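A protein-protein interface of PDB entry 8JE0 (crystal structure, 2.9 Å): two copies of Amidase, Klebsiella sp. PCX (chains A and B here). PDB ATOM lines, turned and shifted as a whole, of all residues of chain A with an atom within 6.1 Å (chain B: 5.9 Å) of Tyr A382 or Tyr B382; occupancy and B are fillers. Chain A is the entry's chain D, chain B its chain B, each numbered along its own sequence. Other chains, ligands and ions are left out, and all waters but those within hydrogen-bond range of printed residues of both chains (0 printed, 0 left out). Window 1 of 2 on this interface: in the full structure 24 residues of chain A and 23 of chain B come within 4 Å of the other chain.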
ATOM      1  N   ILE A  78     -18.222  13.047 -12.413  1.00  0.00           N
ATOM      2  CA  ILE A  78     -17.331  12.727 -13.522  1.00  0.00           C
ATOM      3  C   ILE A  78     -17.569  13.642 -14.716  1.00  0.00           C
ATOM      4  O   ILE A  78     -16.625  14.211 -15.270  1.00  0.00           O
ATOM      5  CB  ILE A  78     -17.491  11.240 -13.907  1.00  0.00           C
ATOM      6  CG1 ILE A  78     -16.903  10.346 -12.813  1.00  0.00           C
ATOM      7  CG2 ILE A  78     -16.835  10.959 -15.246  1.00  0.00           C
ATOM      8  CD1 ILE A  78     -17.083   8.871 -13.068  1.00  0.00           C
ATOM      9  N   VAL A  79     -18.825  13.815 -15.128  1.00  0.00           N
ATOM     10  CA  VAL A  79     -19.119  14.517 -16.373  1.00  0.00           C
ATOM     11  C   VAL A  79     -19.535  15.975 -16.185  1.00  0.00           C
ATOM     12  O   VAL A  79     -19.521  16.738 -17.163  1.00  0.00           O
ATOM     13  CB  VAL A  79     -20.204  13.768 -17.177  1.00  0.00           C
ATOM     14  CG1 VAL A  79     -19.874  12.289 -17.259  1.00  0.00           C
ATOM     15  CG2 VAL A  79     -21.573  13.986 -16.553  1.00  0.00           C
ATOM     16  N   LEU A  81     -18.544  18.239 -13.295  1.00  0.00           N
ATOM     17  CA  LEU A  81     -17.527  19.123 -12.733  1.00  0.00           C
ATOM     18  C   LEU A  81     -16.603  19.745 -13.778  1.00  0.00           C
ATOM     19  O   LEU A  81     -16.330  20.953 -13.668  1.00  0.00           O
ATOM     20  CB  LEU A  81     -16.716  18.364 -11.677  1.00  0.00           C
ATOM     21  CG  LEU A  81     -17.363  18.271 -10.298  1.00  0.00           C
ATOM     22  CD1 LEU A  81     -16.468  17.484  -9.359  1.00  0.00           C
ATOM     23  CD2 LEU A  81     -17.643  19.660  -9.740  1.00  0.00           C
ATOM     24  N   PRO A  82     -16.090  19.022 -14.785  1.00  0.00           N
ATOM     25  CA  PRO A  82     -15.175  19.669 -15.744  1.00  0.00           C
ATOM     26  C   PRO A  82     -15.846  20.672 -16.669  1.00  0.00           C
ATOM     27  O   PRO A  82     -15.134  21.442 -17.327  1.00  0.00           O
ATOM     28  CB  PRO A  82     -14.593  18.494 -16.540  1.00  0.00           C
ATOM     29  CG  PRO A  82     -15.512  17.369 -16.338  1.00  0.00           C
ATOM     30  CD  PRO A  82     -16.241  17.578 -15.052  1.00  0.00           C
ATOM     31  N   ASN A  83     -17.177  20.696 -16.748  1.00  0.00           N
ATOM     32  CA  ASN A  83     -17.881  21.665 -17.577  1.00  0.00           C
ATOM     33  C   ASN A  83     -18.569  22.747 -16.750  1.00  0.00           C
ATOM     34  O   ASN A  83     -19.497  23.399 -17.238  1.00  0.00           O
ATOM     35  CB  ASN A  83     -18.889  20.962 -18.489  1.00  0.00           C
ATOM     36  CG  ASN A  83     -18.270  20.508 -19.801  1.00  0.00           C
ATOM     37  OD1 ASN A  83     -17.418  21.193 -20.374  1.00  0.00           O
ATOM     38  ND2 ASN A  83     -18.699  19.349 -20.287  1.00  0.00           N
ATOM     39  N   LEU A 289     -22.918  15.056 -23.520  1.00  0.00           N
ATOM     40  CA  LEU A 289     -21.713  15.123 -24.346  1.00  0.00           C
ATOM     41  C   LEU A 289     -21.932  14.471 -25.710  1.00  0.00           C
ATOM     42  O   LEU A 289     -21.023  13.865 -26.276  1.00  0.00           O
ATOM     43  CB  LEU A 289     -20.524  14.476 -23.624  1.00  0.00           C
ATOM     44  CG  LEU A 289     -19.547  15.299 -22.775  1.00  0.00           C
ATOM     45  CD1 LEU A 289     -20.167  16.580 -22.250  1.00  0.00           C
ATOM     46  CD2 LEU A 289     -19.013  14.460 -21.616  1.00  0.00           C
ATOM     47  N   TYR A 295     -26.056  18.782 -24.275  1.00  0.00           N
ATOM     48  CA  TYR A 295     -24.671  18.347 -24.400  1.00  0.00           C
ATOM     49  C   TYR A 295     -23.983  18.579 -23.067  1.00  0.00           C
ATOM     50  O   TYR A 295     -23.155  17.780 -22.622  1.00  0.00           O
ATOM     51  CB  TYR A 295     -23.965  19.107 -25.528  1.00  0.00           C
ATOM     52  CG  TYR A 295     -22.516  18.724 -25.751  1.00  0.00           C
ATOM     53  CD1 TYR A 295     -21.501  19.302 -25.000  1.00  0.00           C
ATOM     54  CD2 TYR A 295     -22.162  17.800 -26.727  1.00  0.00           C
ATOM     55  CE1 TYR A 295     -20.178  18.961 -25.201  1.00  0.00           C
ATOM     56  CE2 TYR A 295     -20.837  17.454 -26.939  1.00  0.00           C
ATOM     57  CZ  TYR A 295     -19.851  18.040 -26.172  1.00  0.00           C
ATOM     58  OH  TYR A 295     -18.533  17.705 -26.368  1.00  0.00           O
ATOM     59  N   ASN A 371     -15.520  26.084 -20.548  1.00  0.00           N
ATOM     60  CA  ASN A 371     -15.006  26.070 -19.185  1.00  0.00           C
ATOM     61  C   ASN A 371     -13.538  25.665 -19.189  1.00  0.00           C
ATOM     62  O   ASN A 371     -13.164  24.665 -19.810  1.00  0.00           O
ATOM     63  CB  ASN A 371     -15.824  25.116 -18.313  1.00  0.00           C
ATOM     64  CG  ASN A 371     -15.442  25.191 -16.848  1.00  0.00           C
ATOM     65  OD1 ASN A 371     -15.833  26.119 -16.140  1.00  0.00           O
ATOM     66  ND2 ASN A 371     -14.683  24.203 -16.383  1.00  0.00           N
ATOM     67  N   CYS A 372     -12.709  26.446 -18.492  1.00  0.00           N
ATOM     68  CA  CYS A 372     -11.272  26.215 -18.457  1.00  0.00           C
ATOM     69  C   CYS A 372     -10.751  25.811 -17.088  1.00  0.00           C
ATOM     70  O   CYS A 372      -9.677  25.206 -17.010  1.00  0.00           O
ATOM     71  CB  CYS A 372     -10.524  27.472 -18.923  1.00  0.00           C
ATOM     72  SG  CYS A 372     -11.098  28.117 -20.513  1.00  0.00           S
ATOM     73  N   ALA A 373     -11.475  26.129 -16.018  1.00  0.00           N
ATOM     74  CA  ALA A 373     -11.096  25.717 -14.677  1.00  0.00           C
ATOM     75  C   ALA A 373     -12.348  25.577 -13.827  1.00  0.00           C
ATOM     76  O   ALA A 373     -13.358  26.246 -14.069  1.00  0.00           O
ATOM     77  CB  ALA A 373     -10.123  26.704 -14.023  1.00  0.00           C
ATOM     78  N   THR A 374     -12.274  24.698 -12.831  1.00  0.00           N
ATOM     79  CA  THR A 374     -13.372  24.496 -11.895  1.00  0.00           C
ATOM     80  C   THR A 374     -12.809  24.308 -10.497  1.00  0.00           C
ATOM     81  O   THR A 374     -11.931  23.465 -10.287  1.00  0.00           O
ATOM     82  CB  THR A 374     -14.229  23.284 -12.279  1.00  0.00           C
ATOM     83  OG1 THR A 374     -14.704  23.432 -13.623  1.00  0.00           O
ATOM     84  CG2 THR A 374     -15.421  23.161 -11.338  1.00  0.00           C
ATOM     85  N   ILE A 375     -13.314  25.092  -9.550  1.00  0.00           N
ATOM     86  CA  ILE A 375     -12.974  24.959  -8.140  1.00  0.00           C
ATOM     87  C   ILE A 375     -14.214  24.480  -7.400  1.00  0.00           C
ATOM     88  O   ILE A 375     -15.289  25.077  -7.528  1.00  0.00           O
ATOM     89  CB  ILE A 375     -12.453  26.282  -7.552  1.00  0.00           C
ATOM     90  CG1 ILE A 375     -11.187  26.723  -8.288  1.00  0.00           C
ATOM     91  CG2 ILE A 375     -12.183  26.133  -6.061  1.00  0.00           C
ATOM     92  CD1 ILE A 375     -10.753  28.121  -7.957  1.00  0.00           C
ATOM     93  N   GLN A 379     -11.263  23.233  -3.702  1.00  0.00           N
ATOM     94  CA  GLN A 379     -10.282  22.365  -4.337  1.00  0.00           C
ATOM     95  C   GLN A 379     -10.346  22.539  -5.848  1.00  0.00           C
ATOM     96  O   GLN A 379     -11.436  22.618  -6.427  1.00  0.00           O
ATOM     97  CB  GLN A 379     -10.532  20.898  -3.969  1.00  0.00           C
ATOM     98  CG  GLN A 379      -9.552  19.903  -4.576  1.00  0.00           C
ATOM     99  CD  GLN A 379     -10.050  18.468  -4.479  1.00  0.00           C
ATOM    100  OE1 GLN A 379     -11.120  18.206  -3.926  1.00  0.00           O
ATOM    101  NE2 GLN A 379      -9.278  17.532  -5.023  1.00  0.00           N
ATOM    102  N   ILE A 380      -9.179  22.603  -6.482  1.00  0.00           N
ATOM    103  CA  ILE A 380      -9.106  22.647  -7.938  1.00  0.00           C
ATOM    104  C   ILE A 380      -9.415  21.248  -8.459  1.00  0.00           C
ATOM    105  O   ILE A 380      -8.644  20.310  -8.243  1.00  0.00           O
ATOM    106  CB  ILE A 380      -7.736  23.133  -8.423  1.00  0.00           C
ATOM    107  CG1 ILE A 380      -7.401  24.497  -7.815  1.00  0.00           C
ATOM    108  CG2 ILE A 380      -7.711  23.210  -9.939  1.00  0.00           C
ATOM    109  CD1 ILE A 380      -5.981  24.602  -7.297  1.00  0.00           C
ATOM    110  N   VAL A 381     -10.555  21.101  -9.132  1.00  0.00           N
ATOM    111  CA  VAL A 381     -10.980  19.822  -9.689  1.00  0.00           C
ATOM    112  C   VAL A 381     -10.921  19.805 -11.207  1.00  0.00           C
ATOM    113  O   VAL A 381     -11.244  18.776 -11.822  1.00  0.00           O
ATOM    114  CB  VAL A 381     -12.390  19.446  -9.197  1.00  0.00           C
ATOM    115  CG1 VAL A 381     -12.423  19.431  -7.676  1.00  0.00           C
ATOM    116  CG2 VAL A 381     -13.425  20.415  -9.741  1.00  0.00           C
ATOM    117  N   TYR A 382     -10.509  20.907 -11.829  1.00  0.00           N
ATOM    118  CA  TYR A 382     -10.356  21.003 -13.275  1.00  0.00           C
ATOM    119  C   TYR A 382      -9.581  22.270 -13.597  1.00  0.00           C
ATOM    120  O   TYR A 382      -9.955  23.356 -13.146  1.00  0.00           O
ATOM    121  CB  TYR A 382     -11.719  21.012 -13.969  1.00  0.00           C
ATOM    122  CG  TYR A 382     -11.660  21.105 -15.478  1.00  0.00           C
ATOM    123  CD1 TYR A 382     -11.223  20.031 -16.244  1.00  0.00           C
ATOM    124  CD2 TYR A 382     -12.055  22.261 -16.137  1.00  0.00           C
ATOM    125  CE1 TYR A 382     -11.179  20.109 -17.624  1.00  0.00           C
ATOM    126  CE2 TYR A 382     -12.014  22.348 -17.516  1.00  0.00           C
ATOM    127  CZ  TYR A 382     -11.574  21.270 -18.254  1.00  0.00           C
ATOM    128  OH  TYR A 382     -11.532  21.356 -19.627  1.00  0.00           O
ATOM    129  N   ARG A 383      -8.497  22.152 -14.362  1.00  0.00           N
ATOM    130  CA  ARG A 383      -7.662  23.316 -14.650  1.00  0.00           C
ATOM    131  C   ARG A 383      -6.818  22.991 -15.881  1.00  0.00           C
ATOM    132  O   ARG A 383      -5.807  22.289 -15.772  1.00  0.00           O
ATOM    133  CB  ARG A 383      -6.795  23.675 -13.454  1.00  0.00           C
ATOM    134  CG  ARG A 383      -6.001  24.965 -13.596  1.00  0.00           C
ATOM    135  CD  ARG A 383      -4.820  24.965 -12.634  1.00  0.00           C
ATOM    136  NE  ARG A 383      -4.203  26.277 -12.493  1.00  0.00           N
ATOM    137  CZ  ARG A 383      -3.119  26.516 -11.768  1.00  0.00           C
ATOM    138  NH1 ARG A 383      -2.507  25.551 -11.101  1.00  0.00           N
ATOM    139  NH2 ARG A 383      -2.633  27.754 -11.712  1.00  0.00           N
ATOM    140  N   ARG A 384      -7.247  23.494 -17.036  1.00  0.00           N
ATOM    141  CA  ARG A 384      -6.428  23.396 -18.233  1.00  0.00           C
ATOM    142  C   ARG A 384      -5.096  24.099 -18.007  1.00  0.00           C
ATOM    143  O   ARG A 384      -5.035  25.158 -17.378  1.00  0.00           O
ATOM    144  CB  ARG A 384      -7.155  24.016 -19.426  1.00  0.00           C
ATOM    145  CG  ARG A 384      -8.358  23.228 -19.904  1.00  0.00           C
ATOM    146  CD  ARG A 384      -9.092  23.985 -20.989  1.00  0.00           C
ATOM    147  NE  ARG A 384     -10.346  23.344 -21.361  1.00  0.00           N
ATOM    148  CZ  ARG A 384     -11.202  23.838 -22.246  1.00  0.00           C
ATOM    149  NH1 ARG A 384     -10.969  24.984 -22.867  1.00  0.00           N
ATOM    150  NH2 ARG A 384     -12.319  23.169 -22.513  1.00  0.00           N
ATOM    151  N   VAL B  79     -10.525  14.039 -10.908  1.00  0.00           N
ATOM    152  CA  VAL B  79      -9.412  14.850 -11.396  1.00  0.00           C
ATOM    153  C   VAL B  79      -8.614  14.191 -12.521  1.00  0.00           C
ATOM    154  O   VAL B  79      -7.958  14.907 -13.294  1.00  0.00           O
ATOM    155  CB  VAL B  79      -8.459  15.236 -10.242  1.00  0.00           C
ATOM    156  CG1 VAL B  79      -9.216  15.962  -9.142  1.00  0.00           C
ATOM    157  CG2 VAL B  79      -7.741  14.011  -9.695  1.00  0.00           C
ATOM    158  N   LEU B  81      -9.700  11.559 -14.980  1.00  0.00           N
ATOM    159  CA  LEU B  81     -10.388  11.326 -16.250  1.00  0.00           C
ATOM    160  C   LEU B  81     -10.319  12.507 -17.213  1.00  0.00           C
ATOM    161  O   LEU B  81     -10.038  12.280 -18.401  1.00  0.00           O
ATOM    162  CB  LEU B  81     -11.845  10.926 -15.980  1.00  0.00           C
ATOM    163  CG  LEU B  81     -12.083   9.506 -15.462  1.00  0.00           C
ATOM    164  CD1 LEU B  81     -13.529   9.337 -15.041  1.00  0.00           C
ATOM    165  CD2 LEU B  81     -11.714   8.475 -16.516  1.00  0.00           C
ATOM    166  N   PRO B  82     -10.543  13.762 -16.801  1.00  0.00           N
ATOM    167  CA  PRO B  82     -10.479  14.865 -17.776  1.00  0.00           C
ATOM    168  C   PRO B  82      -9.099  15.070 -18.386  1.00  0.00           C
ATOM    169  O   PRO B  82      -8.994  15.774 -19.400  1.00  0.00           O
ATOM    170  CB  PRO B  82     -10.913  16.093 -16.960  1.00  0.00           C
ATOM    171  CG  PRO B  82     -11.599  15.543 -15.760  1.00  0.00           C
ATOM    172  CD  PRO B  82     -10.894  14.265 -15.459  1.00  0.00           C
ATOM    173  N   ASN B  83      -8.047  14.489 -17.810  1.00  0.00           N
ATOM    174  CA  ASN B  83      -6.700  14.583 -18.359  1.00  0.00           C
ATOM    175  C   ASN B  83      -6.236  13.260 -18.961  1.00  0.00           C
ATOM    176  O   ASN B  83      -5.034  12.989 -19.031  1.00  0.00           O
ATOM    177  CB  ASN B  83      -5.721  15.065 -17.292  1.00  0.00           C
ATOM    178  CG  ASN B  83      -5.996  16.491 -16.862  1.00  0.00           C
ATOM    179  OD1 ASN B  83      -6.256  17.361 -17.697  1.00  0.00           O
ATOM    180  ND2 ASN B  83      -5.950  16.739 -15.556  1.00  0.00           N
ATOM    181  N   LEU B 289      -3.021  19.340 -10.097  1.00  0.00           N
ATOM    182  CA  LEU B 289      -3.469  20.501 -10.876  1.00  0.00           C
ATOM    183  C   LEU B 289      -2.968  21.818 -10.287  1.00  0.00           C
ATOM    184  O   LEU B 289      -3.656  22.841 -10.340  1.00  0.00           O
ATOM    185  CB  LEU B 289      -4.994  20.533 -10.995  1.00  0.00           C
ATOM    186  CG  LEU B 289      -5.761  19.348 -11.569  1.00  0.00           C
ATOM    187  CD1 LEU B 289      -7.240  19.565 -11.319  1.00  0.00           C
ATOM    188  CD2 LEU B 289      -5.485  19.187 -13.052  1.00  0.00           C
ATOM    189  N   ASP B 370      -2.051  17.963 -24.293  1.00  0.00           N
ATOM    190  CA  ASP B 370      -3.344  18.463 -23.842  1.00  0.00           C
ATOM    191  C   ASP B 370      -4.423  17.465 -24.238  1.00  0.00           C
ATOM    192  O   ASP B 370      -4.592  17.166 -25.425  1.00  0.00           O
ATOM    193  CB  ASP B 370      -3.636  19.842 -24.439  1.00  0.00           C
ATOM    194  CG  ASP B 370      -4.889  20.482 -23.862  1.00  0.00           C
ATOM    195  OD1 ASP B 370      -5.456  19.933 -22.893  1.00  0.00           O
ATOM    196  OD2 ASP B 370      -5.303  21.545 -24.372  1.00  0.00           O
ATOM    197  N   ASN B 371      -5.153  16.958 -23.245  1.00  0.00           N
ATOM    198  CA  ASN B 371      -6.231  16.011 -23.496  1.00  0.00           C
ATOM    199  C   ASN B 371      -7.499  16.751 -23.903  1.00  0.00           C
ATOM    200  O   ASN B 371      -7.898  17.724 -23.255  1.00  0.00           O
ATOM    201  CB  ASN B 371      -6.496  15.159 -22.258  1.00  0.00           C
ATOM    202  CG  ASN B 371      -7.292  13.913 -22.574  1.00  0.00           C
ATOM    203  OD1 ASN B 371      -6.763  12.944 -23.115  1.00  0.00           O
ATOM    204  ND2 ASN B 371      -8.579  13.937 -22.248  1.00  0.00           N
ATOM    205  N   CYS B 372      -8.135  16.281 -24.977  1.00  0.00           N
ATOM    206  CA  CYS B 372      -9.344  16.898 -25.505  1.00  0.00           C
ATOM    207  C   CYS B 372     -10.591  16.055 -25.316  1.00  0.00           C
ATOM    208  O   CYS B 372     -11.689  16.610 -25.242  1.00  0.00           O
ATOM    209  CB  CYS B 372      -9.181  17.203 -27.001  1.00  0.00           C
ATOM    210  SG  CYS B 372      -7.926  18.450 -27.378  1.00  0.00           S
ATOM    211  N   ALA B 373     -10.451  14.732 -25.249  1.00  0.00           N
ATOM    212  CA  ALA B 373     -11.581  13.855 -25.003  1.00  0.00           C
ATOM    213  C   ALA B 373     -11.104  12.646 -24.214  1.00  0.00           C
ATOM    214  O   ALA B 373      -9.942  12.243 -24.311  1.00  0.00           O
ATOM    215  CB  ALA B 373     -12.253  13.411 -26.307  1.00  0.00           C
ATOM    216  N   THR B 374     -12.011  12.084 -23.416  1.00  0.00           N
ATOM    217  CA  THR B 374     -11.767  10.849 -22.685  1.00  0.00           C
ATOM    218  C   THR B 374     -12.983   9.947 -22.814  1.00  0.00           C
ATOM    219  O   THR B 374     -14.122  10.400 -22.662  1.00  0.00           O
ATOM    220  CB  THR B 374     -11.478  11.088 -21.194  1.00  0.00           C
ATOM    221  OG1 THR B 374     -10.536  12.157 -21.040  1.00  0.00           O
ATOM    222  CG2 THR B 374     -10.916   9.824 -20.556  1.00  0.00           C
ATOM    223  N   ILE B 375     -12.736   8.674 -23.096  1.00  0.00           N
ATOM    224  CA  ILE B 375     -13.776   7.659 -23.170  1.00  0.00           C
ATOM    225  C   ILE B 375     -13.396   6.565 -22.186  1.00  0.00           C
ATOM    226  O   ILE B 375     -12.322   5.965 -22.306  1.00  0.00           O
ATOM    227  CB  ILE B 375     -13.933   7.100 -24.595  1.00  0.00           C
ATOM    228  CG1 ILE B 375     -14.751   8.063 -25.455  1.00  0.00           C
ATOM    229  CG2 ILE B 375     -14.593   5.729 -24.574  1.00  0.00           C
ATOM    230  CD1 ILE B 375     -14.566   7.851 -26.935  1.00  0.00           C
ATOM    231  N   GLN B 379     -17.841   5.013 -22.521  1.00  0.00           N
ATOM    232  CA  GLN B 379     -18.690   6.166 -22.263  1.00  0.00           C
ATOM    233  C   GLN B 379     -17.892   7.451 -22.435  1.00  0.00           C
ATOM    234  O   GLN B 379     -16.737   7.539 -22.006  1.00  0.00           O
ATOM    235  CB  GLN B 379     -19.287   6.111 -20.854  1.00  0.00           C
ATOM    236  CG  GLN B 379     -19.896   7.432 -20.403  1.00  0.00           C
ATOM    237  CD  GLN B 379     -20.301   7.436 -18.947  1.00  0.00           C
ATOM    238  OE1 GLN B 379     -20.388   8.494 -18.321  1.00  0.00           O
ATOM    239  NE2 GLN B 379     -20.555   6.254 -18.398  1.00  0.00           N
ATOM    240  N   ILE B 380     -18.514   8.445 -23.066  1.00  0.00           N
ATOM    241  CA  ILE B 380     -17.896   9.756 -23.250  1.00  0.00           C
ATOM    242  C   ILE B 380     -17.985  10.491 -21.916  1.00  0.00           C
ATOM    243  O   ILE B 380     -19.010  11.092 -21.594  1.00  0.00           O
ATOM    244  CB  ILE B 380     -18.561  10.547 -24.379  1.00  0.00           C
ATOM    245  CG1 ILE B 380     -18.549   9.733 -25.676  1.00  0.00           C
ATOM    246  CG2 ILE B 380     -17.861  11.885 -24.576  1.00  0.00           C
ATOM    247  CD1 ILE B 380     -19.433  10.300 -26.761  1.00  0.00           C
ATOM    248  N   VAL B 381     -16.906  10.446 -21.129  1.00  0.00           N
ATOM    249  CA  VAL B 381     -16.882  11.140 -19.842  1.00  0.00           C
ATOM    250  C   VAL B 381     -16.290  12.540 -19.934  1.00  0.00           C
ATOM    251  O   VAL B 381     -16.368  13.298 -18.956  1.00  0.00           O
ATOM    252  CB  VAL B 381     -16.102  10.329 -18.787  1.00  0.00           C
ATOM    253  CG1 VAL B 381     -16.692   8.937 -18.653  1.00  0.00           C
ATOM    254  CG2 VAL B 381     -14.630  10.251 -19.148  1.00  0.00           C
ATOM    255  N   TYR B 382     -15.707  12.909 -21.075  1.00  0.00           N
ATOM    256  CA  TYR B 382     -15.057  14.207 -21.231  1.00  0.00           C
ATOM    257  C   TYR B 382     -14.901  14.488 -22.717  1.00  0.00           C
ATOM    258  O   TYR B 382     -14.347  13.660 -23.447  1.00  0.00           O
ATOM    259  CB  TYR B 382     -13.693  14.225 -20.531  1.00  0.00           C
ATOM    260  CG  TYR B 382     -12.954  15.539 -20.650  1.00  0.00           C
ATOM    261  CD1 TYR B 382     -13.380  16.662 -19.954  1.00  0.00           C
ATOM    262  CD2 TYR B 382     -11.826  15.657 -21.455  1.00  0.00           C
ATOM    263  CE1 TYR B 382     -12.707  17.865 -20.057  1.00  0.00           C
ATOM    264  CE2 TYR B 382     -11.145  16.857 -21.563  1.00  0.00           C
ATOM    265  CZ  TYR B 382     -11.591  17.957 -20.862  1.00  0.00           C
ATOM    266  OH  TYR B 382     -10.918  19.153 -20.964  1.00  0.00           O
ATOM    267  N   ARG B 383     -15.384  15.651 -23.163  1.00  0.00           N
ATOM    268  CA  ARG B 383     -15.387  15.966 -24.593  1.00  0.00           C
ATOM    269  C   ARG B 383     -15.598  17.471 -24.755  1.00  0.00           C
ATOM    270  O   ARG B 383     -16.722  17.958 -24.599  1.00  0.00           O
ATOM    271  CB  ARG B 383     -16.465  15.177 -25.319  1.00  0.00           C
ATOM    272  CG  ARG B 383     -16.396  15.266 -26.834  1.00  0.00           C
ATOM    273  CD  ARG B 383     -17.678  14.751 -27.467  1.00  0.00           C
ATOM    274  NE  ARG B 383     -17.702  14.965 -28.909  1.00  0.00           N
ATOM    275  CZ  ARG B 383     -18.660  14.526 -29.714  1.00  0.00           C
ATOM    276  NH1 ARG B 383     -19.702  13.857 -29.250  1.00  0.00           N
ATOM    277  NH2 ARG B 383     -18.566  14.759 -31.020  1.00  0.00           N
ATOM    278  N   ARG B 384     -14.523  18.187 -25.072  1.00  0.00           N
ATOM    279  CA  ARG B 384     -14.659  19.595 -25.416  1.00  0.00           C
ATOM    280  C   ARG B 384     -15.442  19.737 -26.714  1.00  0.00           C
ATOM    281  O   ARG B 384     -15.342  18.899 -27.615  1.00  0.00           O
ATOM    282  CB  ARG B 384     -13.288  20.254 -25.559  1.00  0.00           C
ATOM    283  CG  ARG B 384     -12.309  19.954 -24.441  1.00  0.00           C
ATOM    284  CD  ARG B 384     -11.063  20.811 -24.594  1.00  0.00           C
ATOM    285  NE  ARG B 384     -10.150  20.685 -23.467  1.00  0.00           N
ATOM    286  CZ  ARG B 384      -8.859  20.983 -23.514  1.00  0.00           C
ATOM    287  NH1 ARG B 384      -8.292  21.423 -24.627  1.00  0.00           N
ATOM    288  NH2 ARG B 384      -8.119  20.841 -22.419  1.00  0.00           N
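The guanidinium group (NH1) of Arg A383 sits at hydrogen-bond distance from the backbone carbonyl oxygen (O) of Leu B289, 3.0 Å away. The backbone carbonyl oxygen (O) of Leu A289 sits at hydrogen-bond distance from the guanidinium group (NH1) of Arg B383. The guanidinium group of Arg B384 lies close to the guanidinium group of Arg A384, 3.4 Å away. OH of Tyr A295 sits at hydrogen-bond distance from O of Arg B383, at 2.5 Å. The side-chain hydroxyl (OH) of Tyr A382 lies within hydrogen-bond range of the side-chain hydroxyl (OH) of Tyr B382 (2.6 Å).
OH of Tyr B382 lies within hydrogen-bond range of NE of Arg B384 (3.0 Å). N of Leu A289 sits at hydrogen-bond distance from O of Tyr A295, at 2.9 Å. The backbone carbonyl oxygen (O) of Cys A372 sits at hydrogen-bond distance from the backbone NH (N) of Arg A384. O of Asn A371 lies within hydrogen-bond range of NH2 of Arg A384 (3.2 Å). The backbone NH (N) of Arg B384 lies within hydrogen-bond range of the backbone carbonyl oxygen (O) of Cys B372 (3.2 Å). The backbone carbonyl oxygen (O) of Thr B374 sits at hydrogen-bond distance from the backbone NH (N) of Val B381 (3.2 Å).
Ile A78 touches Leu B81. Val B381 touches Ile A78. Val A79 touches Gln B379. Val A79 touches Val B381 (CA to O, 3.97 Å). Leu A289 touches Ile B380. Leu A289 touches Val B381 (CD2 to C, 3.7 Å). N of Tyr B382 touches CD2 of Leu A289, at 3.7 Å. Tyr A295 touches Arg B384. O of Ile A380 touches CD1 of Leu B289, at 3.5 Å. Leu B289 touches Tyr A382 (CD1 to N, 3.6 Å).
Of the printed residues of chain B, Tyr A382 touches Leu B289 and Tyr B382. Of the printed residues of chain A, Tyr B382 touches Leu A289 (3.7 Å) and Tyr A382 (2.6 Å). Printed residues of chain A within 4 Å of Leu B289: Ile A380 (3.5 Å), Val A381 (3.7 Å), Tyr A382 (3.6 Å) and Arg A383 (3.0 Å). Printed residues of chain A within 4 Å of Leu B81: Ile A78. Leu A81 touches none of the printed residues of chain B. The nearest printed residue of chain B that does not touch Tyr A382 is Pro B82 (4.01 Å). The nearest printed residue of chain B that does not touch Arg A383 is Asn B83 (5.3 Å).
Of the 17 printed residues of chain B, 8 touch a printed residue of chain A. Printed residues of chain B that touch a printed residue of chain A: Leu B81, Leu B289, Gln B379, Ile B380, Val B381, Tyr B382, Arg B383 and Arg B384. Hydrophobic or aromatic side chains of chain B that line the printed part of chain A: Leu B81, Leu B289, Ile B380, Val B381 and Tyr B382. Hydrophobic or aromatic side chains of chain A that line the printed part of chain B: Ile A78, Val A79, Leu A289, Tyr A295, Ile A380 and Tyr A382.
Leu A289 touches Val B381, and with the chains exchanged Val A381 touches Leu B289. Leu A289 touches Tyr B382, and with the chains exchanged Tyr A382 touches Leu B289. Leu A289 touches Arg B383, and with the chains exchanged Arg A383 touches Leu B289. Tyr A382 touches its own counterpart, Tyr B382. 16 positions are printed for both chains.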
